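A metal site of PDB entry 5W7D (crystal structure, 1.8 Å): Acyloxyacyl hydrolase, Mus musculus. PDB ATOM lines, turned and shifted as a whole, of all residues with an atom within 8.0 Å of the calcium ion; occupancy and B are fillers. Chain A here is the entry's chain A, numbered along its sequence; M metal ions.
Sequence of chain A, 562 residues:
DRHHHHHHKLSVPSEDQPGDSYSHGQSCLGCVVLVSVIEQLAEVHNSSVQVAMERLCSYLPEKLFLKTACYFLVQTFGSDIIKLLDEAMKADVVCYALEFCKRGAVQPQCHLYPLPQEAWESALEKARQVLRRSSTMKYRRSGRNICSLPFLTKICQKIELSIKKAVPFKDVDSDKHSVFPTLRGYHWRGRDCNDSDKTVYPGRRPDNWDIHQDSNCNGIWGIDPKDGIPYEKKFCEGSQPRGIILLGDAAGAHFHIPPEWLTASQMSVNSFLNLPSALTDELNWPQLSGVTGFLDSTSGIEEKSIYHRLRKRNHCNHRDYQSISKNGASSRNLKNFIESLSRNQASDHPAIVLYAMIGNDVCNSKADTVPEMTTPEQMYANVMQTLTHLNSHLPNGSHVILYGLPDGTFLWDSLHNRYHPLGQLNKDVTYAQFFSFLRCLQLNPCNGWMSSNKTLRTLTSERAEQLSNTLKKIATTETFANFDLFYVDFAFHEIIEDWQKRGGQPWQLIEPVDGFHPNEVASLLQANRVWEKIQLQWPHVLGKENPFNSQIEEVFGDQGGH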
ATOM      1  N   CYS A 193     -21.887  23.891 -20.845  1.00  0.00           N
ATOM      2  CA  CYS A 193     -22.684  23.139 -19.867  1.00  0.00           C
ATOM      3  C   CYS A 193     -21.898  22.832 -18.598  1.00  0.00           C
ATOM      4  O   CYS A 193     -22.504  22.563 -17.547  1.00  0.00           O
ATOM      5  CB  CYS A 193     -23.237  21.855 -20.533  1.00  0.00           C
ATOM      6  SG  CYS A 193     -22.006  20.692 -21.312  1.00  0.00           S
ATOM      7  N   ARG A 204     -17.337  18.867 -29.030  1.00  0.00           N
ATOM      8  CA  ARG A 204     -16.418  17.801 -28.631  1.00  0.00           C
ATOM      9  C   ARG A 204     -16.982  16.459 -29.056  1.00  0.00           C
ATOM     10  O   ARG A 204     -18.200  16.255 -28.985  1.00  0.00           O
ATOM     11  CB  ARG A 204     -16.236  17.854 -27.103  1.00  0.00           C
ATOM     12  CG  ARG A 204     -15.274  16.888 -26.522  1.00  0.00           C
ATOM     13  CD  ARG A 204     -14.032  17.588 -26.010  1.00  0.00           C
ATOM     14  NE  ARG A 204     -13.040  16.657 -25.468  1.00  0.00           N
ATOM     15  CZ  ARG A 204     -11.782  16.979 -25.227  1.00  0.00           C
ATOM     16  NH1 ARG A 204     -11.375  18.218 -25.478  1.00  0.00           N
ATOM     17  NH2 ARG A 204     -10.921  16.083 -24.736  1.00  0.00           N
ATOM     18  N   ARG A 205     -16.127  15.531 -29.506  1.00  0.00           N
ATOM     19  CA  ARG A 205     -16.575  14.154 -29.647  1.00  0.00           C
ATOM     20  C   ARG A 205     -16.917  13.630 -28.257  1.00  0.00           C
ATOM     21  O   ARG A 205     -16.214  13.943 -27.294  1.00  0.00           O
ATOM     22  CB  ARG A 205     -15.526  13.250 -30.329  1.00  0.00           C
ATOM     23  CG  ARG A 205     -15.267  13.594 -31.816  1.00  0.00           C
ATOM     24  CD  ARG A 205     -14.660  12.432 -32.627  1.00  0.00           C
ATOM     25  NE  ARG A 205     -13.576  11.808 -31.898  1.00  0.00           N
ATOM     26  CZ  ARG A 205     -12.373  12.333 -31.784  1.00  0.00           C
ATOM     27  NH1 ARG A 205     -12.116  13.492 -32.383  1.00  0.00           N
ATOM     28  NH2 ARG A 205     -11.429  11.720 -31.073  1.00  0.00           N
ATOM     29  N   PRO A 206     -18.010  12.905 -28.090  1.00  0.00           N
ATOM     30  CA  PRO A 206     -18.431  12.532 -26.724  1.00  0.00           C
ATOM     31  C   PRO A 206     -17.410  11.652 -26.008  1.00  0.00           C
ATOM     32  O   PRO A 206     -16.699  10.849 -26.604  1.00  0.00           O
ATOM     33  CB  PRO A 206     -19.754  11.781 -26.968  1.00  0.00           C
ATOM     34  CG  PRO A 206     -19.664  11.306 -28.362  1.00  0.00           C
ATOM     35  CD  PRO A 206     -18.960  12.412 -29.102  1.00  0.00           C
ATOM     36  N   ASP A 207     -17.326  11.844 -24.690  1.00  0.00           N
ATOM     37  CA  ASP A 207     -16.444  11.067 -23.829  1.00  0.00           C
ATOM     38  C   ASP A 207     -17.134   9.735 -23.531  1.00  0.00           C
ATOM     39  O   ASP A 207     -18.045   9.655 -22.717  1.00  0.00           O
ATOM     40  CB  ASP A 207     -16.142  11.842 -22.547  1.00  0.00           C
ATOM     41  CG  ASP A 207     -15.318  11.038 -21.541  1.00  0.00           C
ATOM     42  OD1 ASP A 207     -14.547  10.152 -21.941  1.00  0.00           O
ATOM     43  OD2 ASP A 207     -15.436  11.323 -20.336  1.00  0.00           O
ATOM     44  N   TRP A 209     -19.360   8.013 -25.050  1.00  0.00           N
ATOM     45  CA  TRP A 209     -20.802   8.026 -25.326  1.00  0.00           C
ATOM     46  C   TRP A 209     -21.613   8.681 -24.219  1.00  0.00           C
ATOM     47  O   TRP A 209     -22.816   8.454 -24.133  1.00  0.00           O
ATOM     48  CB  TRP A 209     -21.367   6.629 -25.622  1.00  0.00           C
ATOM     49  CG  TRP A 209     -20.725   5.970 -26.833  1.00  0.00           C
ATOM     50  CD1 TRP A 209     -19.986   4.804 -26.837  1.00  0.00           C
ATOM     51  CD2 TRP A 209     -20.754   6.422 -28.196  1.00  0.00           C
ATOM     52  NE1 TRP A 209     -19.565   4.520 -28.116  1.00  0.00           N
ATOM     53  CE2 TRP A 209     -20.020   5.491 -28.967  1.00  0.00           C
ATOM     54  CE3 TRP A 209     -21.335   7.519 -28.840  1.00  0.00           C
ATOM     55  CZ2 TRP A 209     -19.842   5.635 -30.344  1.00  0.00           C
ATOM     56  CZ3 TRP A 209     -21.145   7.667 -30.236  1.00  0.00           C
ATOM     57  CH2 TRP A 209     -20.417   6.720 -30.955  1.00  0.00           C
ATOM     58  N   ASP A 210     -20.983   9.517 -23.383  1.00  0.00           N
ATOM     59  CA  ASP A 210     -21.675  10.410 -22.435  1.00  0.00           C
ATOM     60  C   ASP A 210     -22.565   9.633 -21.452  1.00  0.00           C
ATOM     61  O   ASP A 210     -23.681  10.059 -21.117  1.00  0.00           O
ATOM     62  CB  ASP A 210     -22.470  11.497 -23.182  1.00  0.00           C
ATOM     63  CG  ASP A 210     -21.573  12.653 -23.654  1.00  0.00           C
ATOM     64  OD1 ASP A 210     -20.337  12.553 -23.511  1.00  0.00           O
ATOM     65  OD2 ASP A 210     -22.114  13.654 -24.156  1.00  0.00           O
ATOM     66  N   ILE A 211     -22.042   8.529 -20.921  1.00  0.00           N
ATOM     67  CA  ILE A 211     -22.855   7.693 -20.039  1.00  0.00           C
ATOM     68  C   ILE A 211     -23.209   8.420 -18.747  1.00  0.00           C
ATOM     69  O   ILE A 211     -24.338   8.320 -18.261  1.00  0.00           O
ATOM     70  CB  ILE A 211     -22.131   6.366 -19.760  1.00  0.00           C
ATOM     71  CG1 ILE A 211     -22.076   5.557 -21.059  1.00  0.00           C
ATOM     72  CG2 ILE A 211     -22.825   5.579 -18.613  1.00  0.00           C
ATOM     73  CD1 ILE A 211     -21.261   4.285 -20.953  1.00  0.00           C
ATOM     74  N   GLN A 213     -21.997  11.960 -18.012  1.00  0.00           N
ATOM     75  CA  GLN A 213     -21.990  13.399 -18.150  1.00  0.00           C
ATOM     76  C   GLN A 213     -22.221  13.736 -19.621  1.00  0.00           C
ATOM     77  O   GLN A 213     -21.794  12.998 -20.516  1.00  0.00           O
ATOM     78  CB  GLN A 213     -20.679  14.077 -17.673  1.00  0.00           C
ATOM     79  CG  GLN A 213     -20.625  15.590 -18.036  1.00  0.00           C
ATOM     80  CD  GLN A 213     -19.603  16.470 -17.251  1.00  0.00           C
ATOM     81  OE1 GLN A 213     -19.863  17.661 -16.971  1.00  0.00           O
ATOM     82  NE2 GLN A 213     -18.428  15.889 -16.940  1.00  0.00           N
ATOM     83  N   ASP A 214     -22.906  14.844 -19.846  1.00  0.00           N
ATOM     84  CA  ASP A 214     -23.093  15.362 -21.206  1.00  0.00           C
ATOM     85  C   ASP A 214     -21.853  16.158 -21.588  1.00  0.00           C
ATOM     86  O   ASP A 214     -21.817  17.399 -21.512  1.00  0.00           O
ATOM     87  CB  ASP A 214     -24.344  16.221 -21.287  1.00  0.00           C
ATOM     88  CG  ASP A 214     -24.554  16.828 -22.673  1.00  0.00           C
ATOM     89  OD1 ASP A 214     -25.228  17.881 -22.756  1.00  0.00           O
ATOM     90  OD2 ASP A 214     -24.069  16.252 -23.669  1.00  0.00           O
ATOM     91  N   SER A 215     -20.848  15.443 -22.085  1.00  0.00           N
ATOM     92  CA  SER A 215     -19.536  16.043 -22.308  1.00  0.00           C
ATOM     93  C   SER A 215     -19.504  17.004 -23.482  1.00  0.00           C
ATOM     94  O   SER A 215     -18.598  17.837 -23.545  1.00  0.00           O
ATOM     95  CB  SER A 215     -18.460  14.971 -22.502  1.00  0.00           C
ATOM     96  OG  SER A 215     -18.555  14.338 -23.780  1.00  0.00           O
ATOM     97  N   ASN A 216     -20.453  16.928 -24.409  1.00  0.00           N
ATOM     98  CA  ASN A 216     -20.408  17.816 -25.562  1.00  0.00           C
ATOM     99  C   ASN A 216     -21.618  18.750 -25.603  1.00  0.00           C
ATOM    100  O   ASN A 216     -21.875  19.381 -26.621  1.00  0.00           O
ATOM    101  CB  ASN A 216     -20.262  17.019 -26.865  1.00  0.00           C
ATOM    102  CG  ASN A 216     -21.374  16.000 -27.078  1.00  0.00           C
ATOM    103  OD1 ASN A 216     -22.342  15.942 -26.318  1.00  0.00           O
ATOM    104  ND2 ASN A 216     -21.203  15.157 -28.094  1.00  0.00           N
ATOM    105  N   CYS A 217     -22.305  18.913 -24.476  1.00  0.00           N
ATOM    106  CA  CYS A 217     -23.294  19.963 -24.261  1.00  0.00           C
ATOM    107  C   CYS A 217     -24.452  19.900 -25.262  1.00  0.00           C
ATOM    108  O   CYS A 217     -25.201  20.896 -25.415  1.00  0.00           O
ATOM    109  CB  CYS A 217     -22.649  21.353 -24.308  1.00  0.00           C
ATOM    110  SG  CYS A 217     -21.270  21.511 -23.131  1.00  0.00           S
ATOM    111  N   ASN A 218     -24.654  18.765 -25.938  1.00  0.00           N
ATOM    112  CA  ASN A 218     -25.788  18.674 -26.869  1.00  0.00           C
ATOM    113  C   ASN A 218     -27.059  18.184 -26.170  1.00  0.00           C
ATOM    114  O   ASN A 218     -28.083  17.948 -26.847  1.00  0.00           O
ATOM    115  CB  ASN A 218     -25.455  17.791 -28.085  1.00  0.00           C
ATOM    116  CG  ASN A 218     -25.112  16.397 -27.729  1.00  0.00           C
ATOM    117  OD1 ASN A 218     -25.321  15.971 -26.602  1.00  0.00           O
ATOM    118  ND2 ASN A 218     -24.654  15.631 -28.718  1.00  0.00           N
ATOM    119  N   GLY A 219     -27.051  18.116 -24.847  1.00  0.00           N
ATOM    120  CA  GLY A 219     -28.178  17.686 -24.054  1.00  0.00           C
ATOM    121  C   GLY A 219     -28.436  16.190 -24.052  1.00  0.00           C
ATOM    122  O   GLY A 219     -29.343  15.740 -23.346  1.00  0.00           O
ATOM    123  N   ILE A 220     -27.672  15.406 -24.814  1.00  0.00           N
ATOM    124  CA  ILE A 220     -27.889  13.978 -24.945  1.00  0.00           C
ATOM    125  C   ILE A 220     -26.876  13.258 -24.065  1.00  0.00           C
ATOM    126  O   ILE A 220     -25.677  13.481 -24.203  1.00  0.00           O
ATOM    127  CB  ILE A 220     -27.788  13.531 -26.401  1.00  0.00           C
ATOM    128  CG1 ILE A 220     -28.828  14.252 -27.256  1.00  0.00           C
ATOM    129  CG2 ILE A 220     -27.914  12.039 -26.496  1.00  0.00           C
ATOM    130  CD1 ILE A 220     -28.602  14.119 -28.735  1.00  0.00           C
ATOM    131  N   TRP A 221     -27.344  12.416 -23.155  1.00  0.00           N
ATOM    132  CA  TRP A 221     -26.469  11.695 -22.250  1.00  0.00           C
ATOM    133  C   TRP A 221     -27.288  10.605 -21.576  1.00  0.00           C
ATOM    134  O   TRP A 221     -28.515  10.609 -21.634  1.00  0.00           O
ATOM    135  CB  TRP A 221     -25.846  12.608 -21.189  1.00  0.00           C
ATOM    136  CG  TRP A 221     -26.823  13.022 -20.148  1.00  0.00           C
ATOM    137  CD1 TRP A 221     -27.798  13.984 -20.269  1.00  0.00           C
ATOM    138  CD2 TRP A 221     -26.931  12.507 -18.815  1.00  0.00           C
ATOM    139  NE1 TRP A 221     -28.508  14.084 -19.087  1.00  0.00           N
ATOM    140  CE2 TRP A 221     -27.993  13.192 -18.182  1.00  0.00           C
ATOM    141  CE3 TRP A 221     -26.234  11.530 -18.101  1.00  0.00           C
ATOM    142  CZ2 TRP A 221     -28.376  12.931 -16.863  1.00  0.00           C
ATOM    143  CZ3 TRP A 221     -26.626  11.263 -16.782  1.00  0.00           C
ATOM    144  CH2 TRP A 221     -27.685  11.967 -16.181  1.00  0.00           C
ATOM    145  N   GLY A 222     -26.607   9.708 -20.894  1.00  0.00           N
ATOM    146  CA  GLY A 222     -27.261   8.681 -20.122  1.00  0.00           C
ATOM    147  C   GLY A 222     -27.473   7.403 -20.896  1.00  0.00           C
ATOM    148  O   GLY A 222     -27.023   7.226 -22.028  1.00  0.00           O
ATOM    149  N   TYR A 231     -27.611   6.695 -24.903  1.00  0.00           N
ATOM    150  CA  TYR A 231     -28.424   7.474 -25.843  1.00  0.00           C
ATOM    151  C   TYR A 231     -27.568   8.172 -26.895  1.00  0.00           C
ATOM    152  O   TYR A 231     -27.949   8.222 -28.074  1.00  0.00           O
ATOM    153  CB  TYR A 231     -29.230   8.505 -25.067  1.00  0.00           C
ATOM    154  CG  TYR A 231     -30.446   7.985 -24.343  1.00  0.00           C
ATOM    155  CD1 TYR A 231     -30.564   8.104 -22.964  1.00  0.00           C
ATOM    156  CD2 TYR A 231     -31.525   7.448 -25.036  1.00  0.00           C
ATOM    157  CE1 TYR A 231     -31.695   7.680 -22.286  1.00  0.00           C
ATOM    158  CE2 TYR A 231     -32.667   7.025 -24.370  1.00  0.00           C
ATOM    159  CZ  TYR A 231     -32.741   7.135 -23.002  1.00  0.00           C
ATOM    160  OH  TYR A 231     -33.860   6.715 -22.343  1.00  0.00           O
ATOM    161  N   GLU A 232     -26.411   8.684 -26.512  1.00  0.00           N
ATOM    162  CA  GLU A 232     -25.531   9.334 -27.482  1.00  0.00           C
ATOM    163  C   GLU A 232     -25.038   8.355 -28.531  1.00  0.00           C
ATOM    164  O   GLU A 232     -24.861   8.726 -29.689  1.00  0.00           O
ATOM    165  CB  GLU A 232     -24.376  10.019 -26.750  1.00  0.00           C
ATOM    166  CG  GLU A 232     -23.371  10.796 -27.648  1.00  0.00           C
ATOM    167  CD  GLU A 232     -23.591  12.329 -27.688  1.00  0.00           C
ATOM    168  OE1 GLU A 232     -23.167  12.934 -28.681  1.00  0.00           O
ATOM    169  OE2 GLU A 232     -24.139  12.934 -26.749  1.00  0.00           O
ATOM    170  N   CYS A 236     -26.721   9.168 -31.986  1.00  0.00           N
ATOM    171  CA  CYS A 236     -25.761  10.012 -32.697  1.00  0.00           C
ATOM    172  C   CYS A 236     -24.659   9.248 -33.405  1.00  0.00           C
ATOM    173  O   CYS A 236     -24.067   9.812 -34.329  1.00  0.00           O
ATOM    174  CB  CYS A 236     -25.130  11.037 -31.749  1.00  0.00           C
ATOM    175  SG  CYS A 236     -26.356  12.146 -31.003  1.00  0.00           S
ATOM    176  N   CYS A 316     -28.200  16.225 -32.926  1.00  0.00           N
ATOM    177  CA  CYS A 316     -26.952  16.032 -32.205  1.00  0.00           C
ATOM    178  C   CYS A 316     -26.082  17.278 -32.252  1.00  0.00           C
ATOM    179  O   CYS A 316     -25.196  17.438 -31.409  1.00  0.00           O
ATOM    180  CB  CYS A 316     -26.189  14.817 -32.763  1.00  0.00           C
ATOM    181  SG  CYS A 316     -27.106  13.255 -32.616  1.00  0.00           S
ATOM    182  N   PHE A 556     -35.317  14.011 -24.640  1.00  0.00           N
ATOM    183  CA  PHE A 556     -34.589  15.132 -24.065  1.00  0.00           C
ATOM    184  C   PHE A 556     -35.266  16.486 -24.266  1.00  0.00           C
ATOM    185  O   PHE A 556     -34.761  17.500 -23.762  1.00  0.00           O
ATOM    186  CB  PHE A 556     -33.153  15.176 -24.627  1.00  0.00           C
ATOM    187  CG  PHE A 556     -32.365  13.925 -24.314  1.00  0.00           C
ATOM    188  CD1 PHE A 556     -31.758  13.772 -23.078  1.00  0.00           C
ATOM    189  CD2 PHE A 556     -32.218  12.912 -25.253  1.00  0.00           C
ATOM    190  CE1 PHE A 556     -31.046  12.614 -22.781  1.00  0.00           C
ATOM    191  CE2 PHE A 556     -31.495  11.774 -24.956  1.00  0.00           C
ATOM    192  CZ  PHE A 556     -30.927  11.622 -23.707  1.00  0.00           C
ATOM    193  N   GLN A 559     -33.374  19.765 -25.172  1.00  0.00           N
ATOM    194  CA  GLN A 559     -31.973  19.401 -25.057  1.00  0.00           C
ATOM    195  C   GLN A 559     -31.202  20.399 -24.202  1.00  0.00           C
ATOM    196  O   GLN A 559     -29.991  20.590 -24.354  1.00  0.00           O
ATOM    197  CB  GLN A 559     -31.344  19.241 -26.453  1.00  0.00           C
ATOM    198  CG  GLN A 559     -31.943  18.057 -27.232  1.00  0.00           C
ATOM    199  CD  GLN A 559     -31.445  17.949 -28.660  1.00  0.00           C
ATOM    200  OE1 GLN A 559     -32.219  18.028 -29.592  1.00  0.00           O
ATOM    201  NE2 GLN A 559     -30.140  17.716 -28.837  1.00  0.00           N
HETATM  202 CA    CA M   1     -23.932  14.554 -25.237  1.00  0.00          CA
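The side-chain sulfur of Cys 193 is disulfide-bonded to the side-chain sulfur of Cys 217 (2.1 Å). The backbone carbonyl oxygen (O) of Arg 204 lies close to the side-chain amide nitrogen (ND2) of Asn 216 (3.3 Å). N of Asp 207 is in hydrogen-bond range of OD1 of Asp 210 (3.3 Å). OD2 of Asp 214 lies close to N of Cys 217. SG of Cys 236 is disulfide-bonded to SG of Cys 316, at 2.1 Å. OD1 of Asp 210 sits at hydrogen-bond distance from OG of Ser 215 (2.5 Å). N of Gly 222 is in hydrogen-bond range of O of Asp 210, 3.0 Å away. The side-chain amide nitrogen of Asn 218 lies within hydrogen-bond range of the backbone carbonyl oxygen of Cys 316, at 3.3 Å.
Of the 24 residues printed, 6 come within 4 Å of the calcium ion. Along chain A the residues within 4 Å of the calcium ion span positions 210 to 232. The nearest printed residue that does not touch the calcium ion is Ser 215 (4.5 Å).
The calcium ion is bound by the side-chain carboxylate (OE2) of Glu 232 (2.2 Å). The backbone carbonyl oxygen (O) of Ile 220 is bound to the calcium ion (2.3 Å). The calcium ion is bound by the side-chain carboxylate (OD2) of Asp 210. OD2 of Asp 214 is bound to the calcium ion. The calcium ion is bound by OD1 of Asn 216 (2.4 Å). OD1 of Asn 218 is bound to the calcium ion, at 2.4 Å.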
